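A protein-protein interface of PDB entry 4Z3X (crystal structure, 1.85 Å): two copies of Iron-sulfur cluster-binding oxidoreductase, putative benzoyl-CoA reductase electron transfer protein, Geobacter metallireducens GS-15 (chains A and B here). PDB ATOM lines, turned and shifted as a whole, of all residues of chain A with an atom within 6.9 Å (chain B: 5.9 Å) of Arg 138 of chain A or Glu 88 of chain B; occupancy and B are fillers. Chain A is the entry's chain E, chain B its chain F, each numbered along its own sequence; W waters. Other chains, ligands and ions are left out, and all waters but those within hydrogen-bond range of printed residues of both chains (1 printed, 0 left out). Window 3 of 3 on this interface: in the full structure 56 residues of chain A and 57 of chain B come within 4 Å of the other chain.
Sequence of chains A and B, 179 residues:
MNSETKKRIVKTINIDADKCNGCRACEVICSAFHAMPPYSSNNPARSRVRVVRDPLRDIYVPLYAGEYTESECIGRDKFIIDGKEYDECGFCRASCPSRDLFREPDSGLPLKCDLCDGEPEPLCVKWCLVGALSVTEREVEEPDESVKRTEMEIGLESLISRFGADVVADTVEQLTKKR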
ATOM      1  N   ARG A   8     -38.624  25.424  23.225  1.00  0.00           N
ATOM      2  CA  ARG A   8     -37.440  25.835  22.440  1.00  0.00           C
ATOM      3  C   ARG A   8     -36.623  24.665  21.858  1.00  0.00           C
ATOM      4  O   ARG A   8     -36.771  23.513  22.265  1.00  0.00           O
ATOM      5  CB  ARG A   8     -36.506  26.694  23.291  1.00  0.00           C
ATOM      6  CG  ARG A   8     -35.593  25.896  24.195  1.00  0.00           C
ATOM      7  CD  ARG A   8     -34.974  26.811  25.279  1.00  0.00           C
ATOM      8  NE  ARG A   8     -34.731  26.095  26.529  1.00  0.00           N
ATOM      9  CZ  ARG A   8     -33.581  25.506  26.830  1.00  0.00           C
ATOM     10  NH1 ARG A   8     -32.565  25.578  25.970  1.00  0.00           N
ATOM     11  NH2 ARG A   8     -33.437  24.858  27.986  1.00  0.00           N
ATOM     12  N   ILE A   9     -35.740  24.964  20.917  1.00  0.00           N
ATOM     13  CA  ILE A   9     -34.935  23.917  20.286  1.00  0.00           C
ATOM     14  C   ILE A   9     -33.532  23.794  20.927  1.00  0.00           C
ATOM     15  O   ILE A   9     -32.778  24.748  20.955  1.00  0.00           O
ATOM     16  CB  ILE A   9     -34.795  24.175  18.752  1.00  0.00           C
ATOM     17  CG1 ILE A   9     -36.074  23.779  18.029  1.00  0.00           C
ATOM     18  CG2 ILE A   9     -33.627  23.371  18.141  1.00  0.00           C
ATOM     19  CD1 ILE A   9     -35.822  22.829  16.863  1.00  0.00           C
ATOM     20  N   VAL A  10     -33.186  22.611  21.438  1.00  0.00           N
ATOM     21  CA  VAL A  10     -31.853  22.340  21.891  1.00  0.00           C
ATOM     22  C   VAL A  10     -31.158  21.449  20.836  1.00  0.00           C
ATOM     23  O   VAL A  10     -31.758  20.492  20.304  1.00  0.00           O
ATOM     24  CB  VAL A  10     -31.851  21.648  23.236  1.00  0.00           C
ATOM     25  CG1 VAL A  10     -32.710  22.482  24.246  1.00  0.00           C
ATOM     26  CG2 VAL A  10     -32.485  20.280  23.050  1.00  0.00           C
ATOM     27  N   LYS A  11     -29.908  21.778  20.539  1.00  0.00           N
ATOM     28  CA  LYS A  11     -29.167  20.993  19.567  1.00  0.00           C
ATOM     29  C   LYS A  11     -28.111  20.178  20.292  1.00  0.00           C
ATOM     30  O   LYS A  11     -27.506  20.671  21.246  1.00  0.00           O
ATOM     31  CB  LYS A  11     -28.525  21.883  18.508  1.00  0.00           C
ATOM     32  CG  LYS A  11     -29.487  22.779  17.733  1.00  0.00           C
ATOM     33  CD  LYS A  11     -28.751  24.019  17.250  1.00  0.00           C
ATOM     34  CE  LYS A  11     -29.578  24.859  16.316  1.00  0.00           C
ATOM     35  NZ  LYS A  11     -29.540  24.223  14.965  1.00  0.00           N
ATOM     36  N   THR A  12     -27.902  18.940  19.841  1.00  0.00           N
ATOM     37  CA  THR A  12     -27.061  17.957  20.528  1.00  0.00           C
ATOM     38  C   THR A  12     -25.977  17.436  19.563  1.00  0.00           C
ATOM     39  O   THR A  12     -26.300  16.910  18.485  1.00  0.00           O
ATOM     40  CB  THR A  12     -27.899  16.768  21.051  1.00  0.00           C
ATOM     41  OG1 THR A  12     -28.823  17.242  22.039  1.00  0.00           O
ATOM     42  CG2 THR A  12     -27.015  15.723  21.725  1.00  0.00           C
ATOM     43  N   ILE A  13     -24.708  17.645  19.917  1.00  0.00           N
ATOM     44  CA  ILE A  13     -23.590  17.089  19.145  1.00  0.00           C
ATOM     45  C   ILE A  13     -23.386  15.628  19.564  1.00  0.00           C
ATOM     46  O   ILE A  13     -22.943  15.348  20.691  1.00  0.00           O
ATOM     47  CB  ILE A  13     -22.270  17.884  19.356  1.00  0.00           C
ATOM     48  CG1 ILE A  13     -22.553  19.388  19.526  1.00  0.00           C
ATOM     49  CG2 ILE A  13     -21.334  17.611  18.245  1.00  0.00           C
ATOM     50  CD1 ILE A  13     -21.568  20.110  20.465  1.00  0.00           C
ATOM     51  N   THR A 136     -28.074  16.845  16.057  1.00  0.00           N
ATOM     52  CA  THR A 136     -29.501  16.683  15.959  1.00  0.00           C
ATOM     53  C   THR A 136     -30.217  17.638  16.916  1.00  0.00           C
ATOM     54  O   THR A 136     -29.590  18.308  17.767  1.00  0.00           O
ATOM     55  CB  THR A 136     -29.938  15.215  16.232  1.00  0.00           C
ATOM     56  OG1 THR A 136     -29.463  14.796  17.500  1.00  0.00           O
ATOM     57  CG2 THR A 136     -29.335  14.278  15.212  1.00  0.00           C
ATOM     58  N   GLU A 137     -31.531  17.708  16.728  1.00  0.00           N
ATOM     59  CA  GLU A 137     -32.420  18.626  17.400  1.00  0.00           C
ATOM     60  C   GLU A 137     -33.629  17.933  18.006  1.00  0.00           C
ATOM     61  O   GLU A 137     -34.073  16.841  17.541  1.00  0.00           O
ATOM     62  CB  GLU A 137     -33.002  19.660  16.450  1.00  0.00           C
ATOM     63  CG  GLU A 137     -32.073  20.607  15.775  1.00  0.00           C
ATOM     64  CD  GLU A 137     -32.847  21.440  14.760  1.00  0.00           C
ATOM     65  OE1 GLU A 137     -33.711  20.856  14.056  1.00  0.00           O
ATOM     66  OE2 GLU A 137     -32.633  22.670  14.687  1.00  0.00           O
ATOM     67  N   ARG A 138     -34.154  18.627  19.023  1.00  0.00           N
ATOM     68  CA  ARG A 138     -35.467  18.384  19.580  1.00  0.00           C
ATOM     69  C   ARG A 138     -35.998  19.633  20.276  1.00  0.00           C
ATOM     70  O   ARG A 138     -35.235  20.501  20.732  1.00  0.00           O
ATOM     71  CB  ARG A 138     -35.402  17.244  20.573  1.00  0.00           C
ATOM     72  CG  ARG A 138     -34.686  17.631  21.881  1.00  0.00           C
ATOM     73  CD  ARG A 138     -34.341  16.373  22.710  1.00  0.00           C
ATOM     74  NE  ARG A 138     -34.032  16.681  24.113  1.00  0.00           N
ATOM     75  CZ  ARG A 138     -32.822  16.970  24.549  1.00  0.00           C
ATOM     76  NH1 ARG A 138     -31.810  16.961  23.698  1.00  0.00           N
ATOM     77  NH2 ARG A 138     -32.625  17.226  25.833  1.00  0.00           N
ATOM     78  N   GLU A 139     -37.323  19.685  20.396  1.00  0.00           N
ATOM     79  CA  GLU A 139     -38.040  20.742  21.119  1.00  0.00           C
ATOM     80  C   GLU A 139     -38.104  20.403  22.583  1.00  0.00           C
ATOM     81  O   GLU A 139     -38.300  19.252  22.936  1.00  0.00           O
ATOM     82  CB  GLU A 139     -39.455  20.910  20.561  1.00  0.00           C
ATOM     83  N   VAL A 140     -37.937  21.406  23.433  1.00  0.00           N
ATOM     84  CA  VAL A 140     -38.029  21.225  24.883  1.00  0.00           C
ATOM     85  C   VAL A 140     -38.893  22.332  25.504  1.00  0.00           C
ATOM     86  O   VAL A 140     -38.980  23.431  24.958  1.00  0.00           O
ATOM     87  CB  VAL A 140     -36.638  21.234  25.539  1.00  0.00           C
ATOM     88  CG1 VAL A 140     -35.720  20.240  24.840  1.00  0.00           C
ATOM     89  CG2 VAL A 140     -36.048  22.640  25.513  1.00  0.00           C
ATOM     90  N   ARG B  76     -25.241  20.965  22.975  1.00  0.00           N
ATOM     91  CA  ARG B  76     -24.948  20.013  24.026  1.00  0.00           C
ATOM     92  C   ARG B  76     -24.294  18.790  23.471  1.00  0.00           C
ATOM     93  O   ARG B  76     -24.588  18.390  22.330  1.00  0.00           O
ATOM     94  CB  ARG B  76     -26.223  19.612  24.734  1.00  0.00           C
ATOM     95  CG  ARG B  76     -26.942  20.763  25.459  1.00  0.00           C
ATOM     96  CD  ARG B  76     -28.307  20.291  25.942  1.00  0.00           C
ATOM     97  NE  ARG B  76     -29.115  21.405  26.378  1.00  0.00           N
ATOM     98  CZ  ARG B  76     -30.242  21.311  27.092  1.00  0.00           C
ATOM     99  NH1 ARG B  76     -30.720  20.128  27.484  1.00  0.00           N
ATOM    100  NH2 ARG B  76     -30.869  22.426  27.444  1.00  0.00           N
ATOM    101  N   ASP B  77     -23.460  18.136  24.267  1.00  0.00           N
ATOM    102  CA  ASP B  77     -22.722  16.981  23.744  1.00  0.00           C
ATOM    103  C   ASP B  77     -23.219  15.689  24.364  1.00  0.00           C
ATOM    104  O   ASP B  77     -23.819  15.690  25.427  1.00  0.00           O
ATOM    105  CB  ASP B  77     -21.221  17.144  23.919  1.00  0.00           C
ATOM    106  CG  ASP B  77     -20.767  17.117  25.352  1.00  0.00           C
ATOM    107  OD1 ASP B  77     -21.629  17.215  26.275  1.00  0.00           O
ATOM    108  OD2 ASP B  77     -19.510  17.033  25.558  1.00  0.00           O
ATOM    109  N   LYS B  78     -23.078  14.602  23.608  1.00  0.00           N
ATOM    110  CA  LYS B  78     -23.511  13.278  24.025  1.00  0.00           C
ATOM    111  C   LYS B  78     -22.594  12.225  23.387  1.00  0.00           C
ATOM    112  O   LYS B  78     -22.516  12.173  22.191  1.00  0.00           O
ATOM    113  CB  LYS B  78     -24.961  13.055  23.593  1.00  0.00           C
ATOM    114  CG  LYS B  78     -25.584  11.801  24.086  1.00  0.00           C
ATOM    115  CD  LYS B  78     -27.081  11.813  23.727  1.00  0.00           C
ATOM    116  CE  LYS B  78     -27.567  10.404  23.525  1.00  0.00           C
ATOM    117  NZ  LYS B  78     -28.116   9.970  24.847  1.00  0.00           N
ATOM    118  N   TYR B  86     -23.747   7.381  26.862  1.00  0.00           N
ATOM    119  CA  TYR B  86     -23.831   8.249  28.042  1.00  0.00           C
ATOM    120  C   TYR B  86     -24.934   9.264  27.821  1.00  0.00           C
ATOM    121  O   TYR B  86     -25.455   9.340  26.705  1.00  0.00           O
ATOM    122  CB  TYR B  86     -22.454   8.923  28.321  1.00  0.00           C
ATOM    123  CG  TYR B  86     -21.456   7.931  28.889  1.00  0.00           C
ATOM    124  CD1 TYR B  86     -21.452   7.593  30.241  1.00  0.00           C
ATOM    125  CD2 TYR B  86     -20.553   7.303  28.077  1.00  0.00           C
ATOM    126  CE1 TYR B  86     -20.576   6.649  30.758  1.00  0.00           C
ATOM    127  CE2 TYR B  86     -19.663   6.359  28.585  1.00  0.00           C
ATOM    128  CZ  TYR B  86     -19.655   6.053  29.919  1.00  0.00           C
ATOM    129  OH  TYR B  86     -18.766   5.114  30.416  1.00  0.00           O
ATOM    130  N   ASP B  87     -25.338  10.005  28.874  1.00  0.00           N
ATOM    131  CA  ASP B  87     -26.412  10.982  28.730  1.00  0.00           C
ATOM    132  C   ASP B  87     -25.876  12.215  28.086  1.00  0.00           C
ATOM    133  O   ASP B  87     -24.690  12.513  28.210  1.00  0.00           O
ATOM    134  CB  ASP B  87     -26.965  11.460  30.098  1.00  0.00           C
ATOM    135  CG  ASP B  87     -27.111  10.352  31.120  1.00  0.00           C
ATOM    136  OD1 ASP B  87     -27.711   9.307  30.816  1.00  0.00           O
ATOM    137  OD2 ASP B  87     -26.641  10.562  32.268  1.00  0.00           O
ATOM    138  N   GLU B  88     -26.739  13.006  27.485  1.00  0.00           N
ATOM    139  CA  GLU B  88     -26.348  14.350  27.077  1.00  0.00           C
ATOM    140  C   GLU B  88     -25.734  15.154  28.246  1.00  0.00           C
ATOM    141  O   GLU B  88     -26.214  15.117  29.405  1.00  0.00           O
ATOM    142  CB  GLU B  88     -27.573  15.028  26.456  1.00  0.00           C
ATOM    143  CG  GLU B  88     -27.490  16.489  26.136  1.00  0.00           C
ATOM    144  CD  GLU B  88     -28.875  17.011  25.756  1.00  0.00           C
ATOM    145  OE1 GLU B  88     -29.661  17.501  26.628  1.00  0.00           O
ATOM    146  OE2 GLU B  88     -29.199  16.938  24.565  1.00  0.00           O
ATOM    147  N   CYS B  89     -24.633  15.845  27.953  1.00  0.00           N
ATOM    148  CA  CYS B  89     -23.858  16.594  28.949  1.00  0.00           C
ATOM    149  C   CYS B  89     -23.458  15.719  30.111  1.00  0.00           C
ATOM    150  O   CYS B  89     -23.299  16.206  31.221  1.00  0.00           O
ATOM    151  CB  CYS B  89     -24.632  17.798  29.543  1.00  0.00           C
ATOM    152  SG  CYS B  89     -25.297  19.001  28.441  1.00  0.00           S
ATOM    153  N   GLY B  90     -23.335  14.431  29.890  1.00  0.00           N
ATOM    154  CA  GLY B  90     -23.176  13.550  31.011  1.00  0.00           C
ATOM    155  C   GLY B  90     -21.949  13.641  31.853  1.00  0.00           C
ATOM    156  O   GLY B  90     -21.932  13.021  32.922  1.00  0.00           O
ATOM    157  N   PHE B  91     -20.903  14.335  31.383  1.00  0.00           N
ATOM    158  CA  PHE B  91     -19.713  14.482  32.174  1.00  0.00           C
ATOM    159  C   PHE B  91     -19.503  15.934  32.638  1.00  0.00           C
ATOM    160  O   PHE B  91     -18.461  16.253  33.173  1.00  0.00           O
ATOM    161  CB  PHE B  91     -18.494  13.980  31.338  1.00  0.00           C
ATOM    162  CG  PHE B  91     -18.554  12.523  31.054  1.00  0.00           C
ATOM    163  CD1 PHE B  91     -18.062  11.600  31.987  1.00  0.00           C
ATOM    164  CD2 PHE B  91     -19.132  12.059  29.876  1.00  0.00           C
ATOM    165  CE1 PHE B  91     -18.170  10.245  31.726  1.00  0.00           C
ATOM    166  CE2 PHE B  91     -19.222  10.703  29.619  1.00  0.00           C
ATOM    167  CZ  PHE B  91     -18.714   9.800  30.546  1.00  0.00           C
ATOM    168  N   ARG B  99     -30.119  22.245  33.553  1.00  0.00           N
ATOM    169  CA  ARG B  99     -30.512  21.092  34.363  1.00  0.00           C
ATOM    170  C   ARG B  99     -30.514  21.378  35.888  1.00  0.00           C
ATOM    171  O   ARG B  99     -29.971  22.403  36.362  1.00  0.00           O
ATOM    172  CB  ARG B  99     -29.635  19.890  34.030  1.00  0.00           C
ATOM    173  CG  ARG B  99     -28.210  19.907  34.616  1.00  0.00           C
ATOM    174  CD  ARG B  99     -27.189  20.680  33.747  1.00  0.00           C
ATOM    175  NE  ARG B  99     -25.888  20.728  34.413  1.00  0.00           N
ATOM    176  CZ  ARG B  99     -25.091  19.671  34.478  1.00  0.00           C
ATOM    177  NH1 ARG B  99     -25.449  18.543  33.838  1.00  0.00           N
ATOM    178  NH2 ARG B  99     -23.909  19.750  35.048  1.00  0.00           N
HETATM  179  O   HOH W   1     -33.083  22.052  29.211  1.00  0.00           O
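No position is printed for both chains.
Of chain B, only Arg 76 (3.8 Å) and Glu 88 (2.8 Å) come within 4 Å of Arg 138 of chain A.
Glu 88 of chain B touches two residues of chain A.
Of the printed residues of chain B, Ile 13 of chain A touches Arg 76 (2.5 Å), Asp 77 (3.5 Å) and Lys 78 (3.0 Å).
Printed residues of chain B within 4 Å of Val 10 of chain A: Arg 76 (3.7 Å).
Printed residues of chain B within 4 Å of Arg 8 of chain A: Arg 76.
Of the printed residues of chain B, Lys 11 of chain A touches Arg 76.
Of the printed residues of chain A, Lys 78 of chain B touches Thr 12 (3.9 Å) and Ile 13 (3.0 Å).
The nearest printed residue of chain B that does not touch Arg 138 of chain A is Lys 78 of chain B (7.0 Å).
The nearest residue of chain A that does not touch Glu 88 of chain B is Val 10 of chain A (4.9 Å).
Arg 76 of chain B touches Arg 8 of chain A (NH2 to NH2, 3.6 Å).
Arg 76 of chain B touches Val 10 of chain A (NH2 to CG1, 3.7 Å).
Thr 12 of chain A touches Arg 76 of chain B (CA to O, 3.1 Å).
Thr 12 of chain A touches Lys 78 of chain B (CG2 to CB, 3.9 Å).
Asp 77 of chain B touches Ile 13 of chain A (CA to O, 3.5 Å).
Arg 138 of chain A touches Arg 76 of chain B.
Of the 10 printed residues of chain B, 4 touch a printed residue of chain A.
Among the printed residues, Asp or Glu carboxylates within 4 Å of a Lys or Arg side-chain nitrogen of the other chain: Arg 138 of chain A with Glu 88 of chain B (2.8 Å).
Water W1 lies within hydrogen-bond range of the guanidinium group (NH2) of Arg 76 of chain B (2.9 Å) and the guanidinium group (NH2) of Arg 8 of chain A (3.1 Å).
O of Lys 11 of chain A sits at hydrogen-bond distance from N of Arg 76 of chain B (2.9 Å).
The side-chain carboxylate (OE2) of Glu 88 of chain B is in hydrogen-bond range of the side-chain hydroxyl (OG1) of Thr 12 of chain A, 2.6 Å away.
The backbone carbonyl oxygen (O) of Arg 76 of chain B is in hydrogen-bond range of the backbone NH (N) of Ile 13 of chain A (2.5 Å).
The backbone NH (N) of Lys 78 of chain B is in hydrogen-bond range of the backbone carbonyl oxygen (O) of Ile 13 of chain A, 3.0 Å away.
The side-chain carboxylate of Glu 88 of chain B lies within salt-bridge range of the guanidinium group of Arg 138 of chain A (2.8 Å).
O of Val 140 of chain A is in hydrogen-bond range of N of Arg 8 of chain A.
The side-chain amino group (NZ) of Lys 11 of chain A is in salt-bridge range of the side-chain carboxylate (OE2) of Glu 137 of chain A (3.5 Å).
N of Thr 12 of chain A is in hydrogen-bond range of O of Thr 136 of chain A (2.7 Å).
OG1 of Thr 12 of chain A sits at hydrogen-bond distance from NH1 of Arg 138 of chain A (3.4 Å).
The side-chain carboxylate of Glu 88 of chain B lies within salt-bridge range of the guanidinium group of Arg 76 of chain B (3.0 Å).
O of Asp 77 of chain B lies within hydrogen-bond range of N of Cys 89 of chain B (2.7 Å).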
